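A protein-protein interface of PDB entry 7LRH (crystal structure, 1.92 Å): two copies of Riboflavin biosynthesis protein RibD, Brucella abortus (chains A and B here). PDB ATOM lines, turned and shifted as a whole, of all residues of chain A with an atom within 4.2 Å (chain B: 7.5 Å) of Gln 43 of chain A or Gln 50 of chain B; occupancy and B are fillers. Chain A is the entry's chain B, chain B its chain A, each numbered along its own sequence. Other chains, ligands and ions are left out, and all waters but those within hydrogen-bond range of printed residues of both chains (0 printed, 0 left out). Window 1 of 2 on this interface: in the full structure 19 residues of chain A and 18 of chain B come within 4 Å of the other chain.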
ATOM      1  N   VAL A  39      11.745 -17.169 -24.825  1.00  0.00           N
ATOM      2  CA  VAL A  39      10.913 -15.964 -24.899  1.00  0.00           C
ATOM      3  C   VAL A  39       9.447 -16.360 -24.989  1.00  0.00           C
ATOM      4  O   VAL A  39       8.583 -15.769 -24.330  1.00  0.00           O
ATOM      5  CB  VAL A  39      11.335 -15.055 -26.073  1.00  0.00           C
ATOM      6  CG1 VAL A  39      10.472 -13.797 -26.103  1.00  0.00           C
ATOM      7  CG2 VAL A  39      12.820 -14.716 -26.032  1.00  0.00           C
ATOM      8  N   SER A  40       9.137 -17.440 -25.756  1.00  0.00           N
ATOM      9  CA  SER A  40       7.757 -17.812 -25.883  1.00  0.00           C
ATOM     10  C   SER A  40       7.230 -18.350 -24.574  1.00  0.00           C
ATOM     11  O   SER A  40       6.059 -18.107 -24.245  1.00  0.00           O
ATOM     12  CB  SER A  40       7.560 -18.898 -26.991  1.00  0.00           C
ATOM     13  OG  SER A  40       8.005 -18.422 -28.248  1.00  0.00           O
ATOM     14  N   ARG A  41       8.076 -19.043 -23.797  1.00  0.00           N
ATOM     15  CA  ARG A  41       7.613 -19.559 -22.503  1.00  0.00           C
ATOM     16  C   ARG A  41       7.320 -18.434 -21.555  1.00  0.00           C
ATOM     17  O   ARG A  41       6.262 -18.414 -20.891  1.00  0.00           O
ATOM     18  CB  ARG A  41       8.672 -20.466 -21.871  1.00  0.00           C
ATOM     19  CG  ARG A  41       8.950 -21.753 -22.677  1.00  0.00           C
ATOM     20  CD  ARG A  41       9.038 -22.982 -21.831  1.00  0.00           C
ATOM     21  NE  ARG A  41      10.317 -23.169 -21.148  1.00  0.00           N
ATOM     22  CZ  ARG A  41      10.463 -23.249 -19.824  1.00  0.00           C
ATOM     23  NH1 ARG A  41       9.408 -23.131 -19.022  1.00  0.00           N
ATOM     24  NH2 ARG A  41      11.667 -23.453 -19.294  1.00  0.00           N
ATOM     25  N   ALA A  42       8.236 -17.461 -21.497  1.00  0.00           N
ATOM     26  CA  ALA A  42       8.035 -16.342 -20.580  1.00  0.00           C
ATOM     27  C   ALA A  42       6.782 -15.585 -20.946  1.00  0.00           C
ATOM     28  O   ALA A  42       5.895 -15.420 -20.111  1.00  0.00           O
ATOM     29  CB  ALA A  42       9.245 -15.428 -20.594  1.00  0.00           C
ATOM     30  N   GLN A  43       6.627 -15.225 -22.227  1.00  0.00           N
ATOM     31  CA  GLN A  43       5.412 -14.534 -22.667  1.00  0.00           C
ATOM     32  C   GLN A  43       4.151 -15.319 -22.397  1.00  0.00           C
ATOM     33  O   GLN A  43       3.095 -14.716 -22.178  1.00  0.00           O
ATOM     34  CB  GLN A  43       5.495 -14.144 -24.146  1.00  0.00           C
ATOM     35  CG  GLN A  43       4.231 -13.417 -24.562  1.00  0.00           C
ATOM     36  CD  GLN A  43       4.307 -12.822 -25.936  1.00  0.00           C
ATOM     37  OE1 GLN A  43       5.267 -13.052 -26.688  1.00  0.00           O
ATOM     38  NE2 GLN A  43       3.283 -12.062 -26.293  1.00  0.00           N
ATOM     39  N   SER A  44       4.197 -16.664 -22.478  1.00  0.00           N
ATOM     40  CA  SER A  44       2.989 -17.431 -22.241  1.00  0.00           C
ATOM     41  C   SER A  44       2.528 -17.260 -20.789  1.00  0.00           C
ATOM     42  O   SER A  44       1.368 -16.931 -20.540  1.00  0.00           O
ATOM     43  CB  SER A  44       3.234 -18.915 -22.559  1.00  0.00           C
ATOM     44  OG  SER A  44       2.260 -19.679 -21.892  1.00  0.00           O
ATOM     45  N   HIS A  45       3.478 -17.290 -19.849  1.00  0.00           N
ATOM     46  CA  HIS A  45       3.162 -17.138 -18.429  1.00  0.00           C
ATOM     47  C   HIS A  45       2.849 -15.690 -18.062  1.00  0.00           C
ATOM     48  O   HIS A  45       2.072 -15.446 -17.133  1.00  0.00           O
ATOM     49  CB  HIS A  45       4.320 -17.704 -17.586  1.00  0.00           C
ATOM     50  CG  HIS A  45       4.288 -19.193 -17.453  1.00  0.00           C
ATOM     51  ND1 HIS A  45       3.606 -19.833 -16.440  1.00  0.00           N
ATOM     52  CD2 HIS A  45       4.810 -20.173 -18.229  1.00  0.00           C
ATOM     53  CE1 HIS A  45       3.717 -21.144 -16.595  1.00  0.00           C
ATOM     54  NE2 HIS A  45       4.442 -21.377 -17.678  1.00  0.00           N
ATOM     55  N   ILE A  46       3.394 -14.711 -18.788  1.00  0.00           N
ATOM     56  CA  ILE A  46       2.974 -13.331 -18.508  1.00  0.00           C
ATOM     57  C   ILE A  46       1.548 -13.084 -18.991  1.00  0.00           C
ATOM     58  O   ILE A  46       0.827 -12.275 -18.400  1.00  0.00           O
ATOM     59  CB  ILE A  46       3.986 -12.330 -19.095  1.00  0.00           C
ATOM     60  CG1 ILE A  46       5.317 -12.559 -18.416  1.00  0.00           C
ATOM     61  CG2 ILE A  46       3.554 -10.891 -18.871  1.00  0.00           C
ATOM     62  CD1 ILE A  46       6.391 -11.802 -19.016  1.00  0.00           C
ATOM     63  N   LEU A  47       1.111 -13.720 -20.095  1.00  0.00           N
ATOM     64  CA  LEU A  47      -0.303 -13.590 -20.488  1.00  0.00           C
ATOM     65  C   LEU A  47      -1.235 -14.093 -19.389  1.00  0.00           C
ATOM     66  O   LEU A  47      -2.350 -13.574 -19.206  1.00  0.00           O
ATOM     67  CB  LEU A  47      -0.594 -14.367 -21.800  1.00  0.00           C
ATOM     68  CG  LEU A  47       0.072 -13.793 -23.038  1.00  0.00           C
ATOM     69  CD1 LEU A  47      -0.184 -14.794 -24.242  1.00  0.00           C
ATOM     70  CD2 LEU A  47      -0.406 -12.383 -23.350  1.00  0.00           C
ATOM     71  N   PHE A 180       1.946 -19.053 -31.184  1.00  0.00           N
ATOM     72  CA  PHE A 180       3.287 -19.567 -31.055  1.00  0.00           C
ATOM     73  C   PHE A 180       3.398 -20.761 -31.995  1.00  0.00           C
ATOM     74  O   PHE A 180       2.563 -21.657 -31.926  1.00  0.00           O
ATOM     75  CB  PHE A 180       3.547 -20.022 -29.640  1.00  0.00           C
ATOM     76  CG  PHE A 180       3.488 -18.889 -28.625  1.00  0.00           C
ATOM     77  CD1 PHE A 180       4.510 -18.016 -28.560  1.00  0.00           C
ATOM     78  CD2 PHE A 180       2.399 -18.713 -27.802  1.00  0.00           C
ATOM     79  CE1 PHE A 180       4.510 -16.940 -27.666  1.00  0.00           C
ATOM     80  CE2 PHE A 180       2.392 -17.646 -26.867  1.00  0.00           C
ATOM     81  CZ  PHE A 180       3.431 -16.781 -26.812  1.00  0.00           C
ATOM     82  N   ARG A 209       2.798  -7.813 -34.380  1.00  0.00           N
ATOM     83  CA  ARG A 209       4.210  -8.076 -34.203  1.00  0.00           C
ATOM     84  C   ARG A 209       4.484  -9.512 -34.600  1.00  0.00           C
ATOM     85  O   ARG A 209       3.579 -10.355 -34.584  1.00  0.00           O
ATOM     86  CB  ARG A 209       4.669  -7.779 -32.773  1.00  0.00           C
ATOM     87  CG  ARG A 209       3.908  -8.428 -31.611  1.00  0.00           C
ATOM     88  CD  ARG A 209       4.758  -8.199 -30.337  1.00  0.00           C
ATOM     89  NE  ARG A 209       6.048  -8.863 -30.472  1.00  0.00           N
ATOM     90  CZ  ARG A 209       6.265 -10.139 -30.155  1.00  0.00           C
ATOM     91  NH1 ARG A 209       5.279 -10.878 -29.642  1.00  0.00           N
ATOM     92  NH2 ARG A 209       7.464 -10.676 -30.326  1.00  0.00           N
ATOM     93  N   GLU A 220       1.481 -12.064 -33.460  1.00  0.00           N
ATOM     94  CA  GLU A 220       0.316 -11.490 -32.796  1.00  0.00           C
ATOM     95  C   GLU A 220      -0.525 -10.707 -33.799  1.00  0.00           C
ATOM     96  O   GLU A 220       0.010 -10.034 -34.673  1.00  0.00           O
ATOM     97  CB  GLU A 220       0.757 -10.556 -31.625  1.00  0.00           C
ATOM     98  CG  GLU A 220       1.580 -11.283 -30.603  1.00  0.00           C
ATOM     99  CD  GLU A 220       1.733 -10.493 -29.275  1.00  0.00           C
ATOM    100  OE1 GLU A 220       0.702 -10.080 -28.664  1.00  0.00           O
ATOM    101  OE2 GLU A 220       2.906 -10.287 -28.875  1.00  0.00           O
ATOM    102  N   GLU B  12      10.485  -2.211 -37.094  1.00  0.00           N
ATOM    103  CA  GLU B  12       9.319  -1.902 -36.262  1.00  0.00           C
ATOM    104  C   GLU B  12       9.804  -1.145 -35.037  1.00  0.00           C
ATOM    105  O   GLU B  12      10.854  -1.465 -34.487  1.00  0.00           O
ATOM    106  CB  GLU B  12       8.586  -3.170 -35.822  1.00  0.00           C
ATOM    107  CG  GLU B  12       7.140  -2.939 -35.478  1.00  0.00           C
ATOM    108  CD  GLU B  12       6.708  -3.803 -34.287  1.00  0.00           C
ATOM    109  OE1 GLU B  12       5.522  -3.717 -33.863  1.00  0.00           O
ATOM    110  OE2 GLU B  12       7.580  -4.571 -33.785  1.00  0.00           O
ATOM    111  N   ILE B  14       8.853   0.212 -31.274  1.00  0.00           N
ATOM    112  CA  ILE B  14       8.014   0.214 -30.078  1.00  0.00           C
ATOM    113  C   ILE B  14       8.563   1.276 -29.131  1.00  0.00           C
ATOM    114  O   ILE B  14       9.724   1.213 -28.794  1.00  0.00           O
ATOM    115  CB  ILE B  14       8.032  -1.133 -29.348  1.00  0.00           C
ATOM    116  CG1 ILE B  14       7.583  -2.247 -30.293  1.00  0.00           C
ATOM    117  CG2 ILE B  14       7.123  -1.038 -28.089  1.00  0.00           C
ATOM    118  CD1 ILE B  14       7.597  -3.601 -29.604  1.00  0.00           C
ATOM    119  N   GLN B  43       6.886  -7.734 -17.862  1.00  0.00           N
ATOM    120  CA  GLN B  43       6.607  -7.350 -19.239  1.00  0.00           C
ATOM    121  C   GLN B  43       7.699  -6.447 -19.773  1.00  0.00           C
ATOM    122  O   GLN B  43       8.105  -6.565 -20.937  1.00  0.00           O
ATOM    123  CB  GLN B  43       5.248  -6.686 -19.354  1.00  0.00           C
ATOM    124  CG  GLN B  43       5.061  -6.051 -20.715  1.00  0.00           C
ATOM    125  CD  GLN B  43       3.626  -6.004 -21.129  1.00  0.00           C
ATOM    126  OE1 GLN B  43       3.102  -6.958 -21.749  1.00  0.00           O
ATOM    127  NE2 GLN B  43       2.946  -4.907 -20.779  1.00  0.00           N
ATOM    128  N   SER B  44       8.238  -5.569 -18.906  1.00  0.00           N
ATOM    129  CA  SER B  44       9.279  -4.673 -19.313  1.00  0.00           C
ATOM    130  C   SER B  44      10.509  -5.454 -19.747  1.00  0.00           C
ATOM    131  O   SER B  44      11.110  -5.164 -20.790  1.00  0.00           O
ATOM    132  CB  SER B  44       9.616  -3.730 -18.121  1.00  0.00           C
ATOM    133  OG  SER B  44      10.482  -2.736 -18.531  1.00  0.00           O
ATOM    134  N   HIS B  45      10.860  -6.508 -19.025  1.00  0.00           N
ATOM    135  CA  HIS B  45      12.045  -7.236 -19.465  1.00  0.00           C
ATOM    136  C   HIS B  45      11.770  -8.102 -20.682  1.00  0.00           C
ATOM    137  O   HIS B  45      12.690  -8.394 -21.457  1.00  0.00           O
ATOM    138  CB  HIS B  45      12.584  -8.057 -18.315  1.00  0.00           C
ATOM    139  CG  HIS B  45      13.424  -7.228 -17.407  1.00  0.00           C
ATOM    140  ND1 HIS B  45      14.793  -7.187 -17.506  1.00  0.00           N
ATOM    141  CD2 HIS B  45      13.081  -6.304 -16.475  1.00  0.00           C
ATOM    142  CE1 HIS B  45      15.270  -6.312 -16.630  1.00  0.00           C
ATOM    143  NE2 HIS B  45      14.250  -5.764 -15.990  1.00  0.00           N
ATOM    144  N   ILE B  46      10.517  -8.494 -20.857  1.00  0.00           N
ATOM    145  CA  ILE B  46      10.135  -9.294 -22.026  1.00  0.00           C
ATOM    146  C   ILE B  46      10.231  -8.473 -23.294  1.00  0.00           C
ATOM    147  O   ILE B  46      10.703  -8.956 -24.324  1.00  0.00           O
ATOM    148  CB  ILE B  46       8.717  -9.816 -21.794  1.00  0.00           C
ATOM    149  CG1 ILE B  46       8.823 -11.050 -20.950  1.00  0.00           C
ATOM    150  CG2 ILE B  46       8.032 -10.190 -23.078  1.00  0.00           C
ATOM    151  CD1 ILE B  46       9.094 -12.262 -21.871  1.00  0.00           C
ATOM    152  N   LEU B  47       9.833  -7.199 -23.224  1.00  0.00           N
ATOM    153  CA  LEU B  47       9.991  -6.296 -24.356  1.00  0.00           C
ATOM    154  C   LEU B  47      11.446  -6.198 -24.789  1.00  0.00           C
ATOM    155  O   LEU B  47      11.745  -6.119 -25.992  1.00  0.00           O
ATOM    156  CB  LEU B  47       9.428  -4.923 -23.977  1.00  0.00           C
ATOM    157  CG  LEU B  47       7.919  -4.922 -23.803  1.00  0.00           C
ATOM    158  CD1 LEU B  47       7.515  -3.584 -23.099  1.00  0.00           C
ATOM    159  CD2 LEU B  47       7.134  -5.103 -25.096  1.00  0.00           C
ATOM    160  N   ARG B  48      12.378  -6.174 -23.814  1.00  0.00           N
ATOM    161  CA  ARG B  48      13.800  -6.115 -24.155  1.00  0.00           C
ATOM    162  C   ARG B  48      14.247  -7.386 -24.878  1.00  0.00           C
ATOM    163  O   ARG B  48      15.024  -7.326 -25.839  1.00  0.00           O
ATOM    164  CB  ARG B  48      14.610  -5.909 -22.877  1.00  0.00           C
ATOM    165  CG  ARG B  48      14.345  -4.545 -22.268  1.00  0.00           C
ATOM    166  CD  ARG B  48      15.153  -4.400 -20.979  1.00  0.00           C
ATOM    167  NE  ARG B  48      15.268  -2.981 -20.605  1.00  0.00           N
ATOM    168  CZ  ARG B  48      15.950  -2.522 -19.547  1.00  0.00           C
ATOM    169  NH1 ARG B  48      16.589  -3.355 -18.725  1.00  0.00           N
ATOM    170  NH2 ARG B  48      15.964  -1.210 -19.309  1.00  0.00           N
ATOM    171  N   ALA B  49      13.808  -8.543 -24.378  1.00  0.00           N
ATOM    172  CA  ALA B  49      14.142  -9.817 -25.030  1.00  0.00           C
ATOM    173  C   ALA B  49      13.562  -9.948 -26.435  1.00  0.00           C
ATOM    174  O   ALA B  49      14.146 -10.648 -27.273  1.00  0.00           O
ATOM    175  CB  ALA B  49      13.687 -10.973 -24.166  1.00  0.00           C
ATOM    176  N   GLN B  50      12.398  -9.361 -26.699  1.00  0.00           N
ATOM    177  CA  GLN B  50      11.814  -9.398 -28.043  1.00  0.00           C
ATOM    178  C   GLN B  50      12.419  -8.376 -29.007  1.00  0.00           C
ATOM    179  O   GLN B  50      12.185  -8.457 -30.224  1.00  0.00           O
ATOM    180  CB  GLN B  50      10.290  -9.194 -27.952  1.00  0.00           C
ATOM    181  CG  GLN B  50       9.565 -10.222 -27.129  1.00  0.00           C
ATOM    182  CD  GLN B  50       8.078  -9.840 -26.790  1.00  0.00           C
ATOM    183  OE1 GLN B  50       7.746  -8.674 -26.653  1.00  0.00           O
ATOM    184  NE2 GLN B  50       7.195 -10.852 -26.722  1.00  0.00           N
ATOM    185  N   ALA B  51      13.197  -7.420 -28.522  1.00  0.00           N
ATOM    186  CA  ALA B  51      13.738  -6.364 -29.367  1.00  0.00           C
ATOM    187  C   ALA B  51      15.113  -6.759 -29.888  1.00  0.00           C
ATOM    188  O   ALA B  51      15.897  -7.426 -29.208  1.00  0.00           O
ATOM    189  CB  ALA B  51      13.871  -5.033 -28.594  1.00  0.00           C
ATOM    190  N   ASP B  52      15.409  -6.323 -31.097  1.00  0.00           N
ATOM    191  CA  ASP B  52      16.782  -6.432 -31.620  1.00  0.00           C
ATOM    192  C   ASP B  52      17.702  -5.380 -30.992  1.00  0.00           C
ATOM    193  O   ASP B  52      18.902  -5.621 -30.774  1.00  0.00           O
ATOM    194  CB  ASP B  52      16.776  -6.241 -33.123  1.00  0.00           C
ATOM    195  CG  ASP B  52      16.295  -7.496 -33.864  1.00  0.00           C
ATOM    196  OD1 ASP B  52      16.422  -8.605 -33.301  1.00  0.00           O
ATOM    197  OD2 ASP B  52      15.762  -7.358 -34.975  1.00  0.00           O
ATOM    198  N   ILE B  53      17.144  -4.204 -30.751  1.00  0.00           N
ATOM    199  CA  ILE B  53      17.881  -3.017 -30.293  1.00  0.00           C
ATOM    200  C   ILE B  53      17.042  -2.349 -29.233  1.00  0.00           C
ATOM    201  O   ILE B  53      15.823  -2.237 -29.385  1.00  0.00           O
ATOM    202  CB  ILE B  53      18.179  -2.016 -31.434  1.00  0.00           C
ATOM    203  CG1 ILE B  53      19.338  -2.517 -32.291  1.00  0.00           C
ATOM    204  CG2 ILE B  53      18.497  -0.580 -30.922  1.00  0.00           C
ATOM    205  CD1 ILE B  53      20.029  -1.454 -33.146  1.00  0.00           C
ATOM    206  N   CYS B  70      18.458  -7.746 -20.332  1.00  0.00           N
ATOM    207  CA  CYS B  70      17.292  -8.553 -19.975  1.00  0.00           C
ATOM    208  C   CYS B  70      17.624  -9.372 -18.746  1.00  0.00           C
ATOM    209  O   CYS B  70      18.593 -10.135 -18.780  1.00  0.00           O
ATOM    210  CB  CYS B  70      16.872  -9.500 -21.134  1.00  0.00           C
ATOM    211  SG  CYS B  70      15.333 -10.412 -20.761  1.00  0.00           S
ATOM    212  N   LEU B  72      15.256 -11.462 -16.917  1.00  0.00           N
ATOM    213  CA  LEU B  72      14.429 -12.624 -16.621  1.00  0.00           C
ATOM    214  C   LEU B  72      15.287 -13.874 -16.661  1.00  0.00           C
ATOM    215  O   LEU B  72      16.045 -14.062 -17.614  1.00  0.00           O
ATOM    216  CB  LEU B  72      13.307 -12.752 -17.619  1.00  0.00           C
ATOM    217  CG  LEU B  72      12.243 -11.702 -17.401  1.00  0.00           C
ATOM    218  CD1 LEU B  72      11.605 -11.375 -18.732  1.00  0.00           C
ATOM    219  CD2 LEU B  72      11.267 -12.221 -16.431  1.00  0.00           C
ATOM    220  N   LEU B  75      16.609 -15.730 -19.897  1.00  0.00           N
ATOM    221  CA  LEU B  75      16.526 -14.840 -21.044  1.00  0.00           C
ATOM    222  C   LEU B  75      17.679 -13.860 -21.119  1.00  0.00           C
ATOM    223  O   LEU B  75      17.691 -13.017 -22.030  1.00  0.00           O
ATOM    224  CB  LEU B  75      15.188 -14.083 -21.020  1.00  0.00           C
ATOM    225  CG  LEU B  75      13.957 -14.948 -21.316  1.00  0.00           C
ATOM    226  CD1 LEU B  75      12.732 -14.131 -21.528  1.00  0.00           C
ATOM    227  CD2 LEU B  75      14.290 -15.731 -22.560  1.00  0.00           C
ATOM    228  N   ARG B  78      19.225 -13.083 -24.295  1.00  0.00           N
ATOM    229  CA  ARG B  78      18.463 -12.308 -25.255  1.00  0.00           C
ATOM    230  C   ARG B  78      18.550 -10.820 -24.973  1.00  0.00           C
ATOM    231  O   ARG B  78      17.764 -10.046 -25.541  1.00  0.00           O
ATOM    232  CB  ARG B  78      16.991 -12.757 -25.262  1.00  0.00           C
ATOM    233  CG  ARG B  78      16.801 -14.293 -25.334  1.00  0.00           C
ATOM    234  CD  ARG B  78      17.466 -14.944 -26.553  1.00  0.00           C
ATOM    235  NE  ARG B  78      16.533 -15.820 -27.278  1.00  0.00           N
ATOM    236  CZ  ARG B  78      16.568 -17.161 -27.313  1.00  0.00           C
ATOM    237  NH1 ARG B  78      15.643 -17.828 -28.029  1.00  0.00           N
ATOM    238  NH2 ARG B  78      17.503 -17.834 -26.628  1.00  0.00           N
ATOM    239  N   PRO B  80      19.419  -7.276 -25.767  1.00  0.00           N
ATOM    240  CA  PRO B  80      19.579  -6.734 -27.111  1.00  0.00           C
ATOM    241  C   PRO B  80      20.821  -5.843 -27.262  1.00  0.00           C
ATOM    242  O   PRO B  80      21.541  -5.566 -26.307  1.00  0.00           O
ATOM    243  CB  PRO B  80      18.308  -5.902 -27.259  1.00  0.00           C
ATOM    244  CG  PRO B  80      18.032  -5.433 -25.846  1.00  0.00           C
ATOM    245  CD  PRO B  80      18.281  -6.668 -25.043  1.00  0.00           C
ATOM    246  N   ALA B 154      15.543  -5.679 -37.050  1.00  0.00           N
ATOM    247  CA  ALA B 154      14.128  -5.750 -37.433  1.00  0.00           C
ATOM    248  C   ALA B 154      13.174  -5.017 -36.477  1.00  0.00           C
ATOM    249  O   ALA B 154      12.073  -4.644 -36.893  1.00  0.00           O
ATOM    250  CB  ALA B 154      13.657  -7.204 -37.513  1.00  0.00           C
ATOM    251  N   SER B 155      13.565  -4.781 -35.231  1.00  0.00           N
ATOM    252  CA  SER B 155      12.685  -4.140 -34.248  1.00  0.00           C
ATOM    253  C   SER B 155      13.531  -3.366 -33.267  1.00  0.00           C
ATOM    254  O   SER B 155      14.557  -3.862 -32.815  1.00  0.00           O
ATOM    255  CB  SER B 155      11.859  -5.172 -33.490  1.00  0.00           C
ATOM    256  OG  SER B 155      12.747  -6.073 -32.856  1.00  0.00           O
ATOM    257  N   VAL B 156      13.090  -2.144 -32.964  1.00  0.00           N
ATOM    258  CA  VAL B 156      13.765  -1.221 -32.060  1.00  0.00           C
ATOM    259  C   VAL B 156      12.801  -0.965 -30.910  1.00  0.00           C
ATOM    260  O   VAL B 156      11.612  -0.737 -31.152  1.00  0.00           O
ATOM    261  CB  VAL B 156      14.117   0.102 -32.750  1.00  0.00           C
ATOM    262  CG1 VAL B 156      14.676   1.181 -31.645  1.00  0.00           C
ATOM    263  CG2 VAL B 156      15.073  -0.127 -33.957  1.00  0.00           C
ATOM    264  N   LEU B 157      13.285  -1.089 -29.672  1.00  0.00           N
ATOM    265  CA  LEU B 157      12.517  -0.703 -28.491  1.00  0.00           C
ATOM    266  C   LEU B 157      13.100   0.628 -28.014  1.00  0.00           C
ATOM    267  O   LEU B 157      14.279   0.680 -27.702  1.00  0.00           O
ATOM    268  CB  LEU B 157      12.649  -1.748 -27.388  1.00  0.00           C
ATOM    269  CG  LEU B 157      12.100  -1.504 -25.978  1.00  0.00           C
ATOM    270  CD1 LEU B 157      10.648  -1.310 -25.969  1.00  0.00           C
ATOM    271  CD2 LEU B 157      12.499  -2.645 -25.080  1.00  0.00           C
ATOM    272  N   ARG B 176       4.074   0.931 -32.169  1.00  0.00           N
ATOM    273  CA  ARG B 176       3.380   0.487 -30.971  1.00  0.00           C
ATOM    274  C   ARG B 176       3.840   1.341 -29.792  1.00  0.00           C
ATOM    275  O   ARG B 176       4.998   1.770 -29.729  1.00  0.00           O
ATOM    276  CB  ARG B 176       3.583  -0.984 -30.624  1.00  0.00           C
ATOM    277  CG  ARG B 176       3.616  -1.876 -31.874  1.00  0.00           C
ATOM    278  CD  ARG B 176       3.473  -3.373 -31.593  1.00  0.00           C
ATOM    279  NE  ARG B 176       4.414  -3.891 -30.594  1.00  0.00           N
ATOM    280  CZ  ARG B 176       4.068  -4.185 -29.333  1.00  0.00           C
ATOM    281  NH1 ARG B 176       2.810  -4.010 -28.906  1.00  0.00           N
ATOM    282  NH2 ARG B 176       4.964  -4.685 -28.489  1.00  0.00           N
ATOM    283  N   ILE B 178       3.644   1.546 -25.556  1.00  0.00           N
ATOM    284  CA  ILE B 178       3.319   0.870 -24.296  1.00  0.00           C
ATOM    285  C   ILE B 178       3.622   1.847 -23.174  1.00  0.00           C
ATOM    286  O   ILE B 178       4.751   2.333 -23.088  1.00  0.00           O
ATOM    287  CB  ILE B 178       4.109  -0.415 -24.080  1.00  0.00           C
ATOM    288  CG1 ILE B 178       4.013  -1.257 -25.362  1.00  0.00           C
ATOM    289  CG2 ILE B 178       3.541  -1.138 -22.854  1.00  0.00           C
ATOM    290  CD1 ILE B 178       4.892  -2.462 -25.392  1.00  0.00           C
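The side-chain amide nitrogen (NE2) of Gln 50 of chain B is in hydrogen-bond range of the side-chain amide oxygen (OE1) of Gln 43 of chain A (2.9 Å). The guanidinium group (NH1) of Arg 209 of chain A lies close to the side-chain amide nitrogen (NE2) of Gln 50 of chain B, 3.5 Å away.
Gln 43 of chain A touches Ile 46 of chain B, but with the chains exchanged Ile 46 of chain A does not touch Gln 43 of chain B (4.3 Å). Ile 46 of chain A touches its own counterpart, Ile 46 of chain B. Positions printed for both chains: 43, 44, 45, 46 and 47. Of the 9 pairs that touch across the chains among the printed residues, 1 has its exchanged pair printed and touching as well.
NE2 of Gln 43 of chain A sits at hydrogen-bond distance from OE2 of Glu 220 of chain A (3.2 Å). The guanidinium group (NE) of Arg 176 of chain B lies within salt-bridge range of the side-chain carboxylate (OE1) of Glu 12 of chain B (3.5 Å). The side-chain sulfur (SG) of Cys 70 of chain B sits close to the backbone carbonyl oxygen (O) of Leu 75 of chain B (3.7 Å). The guanidinium group of Arg 209 of chain A is in salt-bridge range of the side-chain carboxylate of Glu 220 of chain A.
Of chain B, only Ile 46 (3.9 Å) and Gln 50 (2.9 Å) come within 4 Å of Gln 43 of chain A. Of chain A, only Val 39 (3.8 Å), Gln 43 (2.9 Å) and Arg 209 (3.5 Å) come within 4 Å of Gln 50 of chain B. Of the printed residues of chain B, Ala 42 of chain A touches Ile 46 and Leu 75. Printed residues of chain B within 4 Å of Ile 46 of chain A: Ile 46 (3.2 Å). Printed residues of chain A within 4 Å of Ile 46 of chain B: Ala 42, Gln 43 and Ile 46. Printed residues of chain A within 4 Å of Arg 176 of chain B: Arg 209 (3.98 Å). The nearest residue of chain B that does not touch Gln 43 of chain A is Leu 75 of chain B (6.2 Å). The nearest printed residue of chain A that does not touch Gln 50 of chain B is Glu 220 of chain A (4.8 Å). The nearest printed residue of chain A that does not touch Arg 176 of chain B is Glu 220 of chain A (6.0 Å).
CG1 of Val 39 of chain A touches CG of Gln 50 of chain B, 3.8 Å away. CD2 of Leu 75 of chain B touches N of Val 39 of chain A (3.7 Å). CD1 of Ile 46 of chain B touches CB of Ala 42 of chain A, 3.4 Å away. CD1 of Leu 75 of chain B touches CB of Ala 42 of chain A, 3.8 Å away. N of Gln 43 of chain A touches CD1 of Ile 46 of chain B (3.9 Å). Ile 46 of chain B touches Ile 46 of chain A (CG1 to CD1, 3.2 Å). NH2 of Arg 176 of chain B touches CD of Arg 209 of chain A, 3.98 Å away.
Printed residues of chain A that touch a printed residue of chain B: Val 39, Ala 42, Gln 43, Ile 46 and Arg 209. Hydrophobic or aromatic side chains of chain A that line the printed part of chain B: Val 39, Ala 42 and Ile 46. Among the printed residues, 9 pairs touch across the chains.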
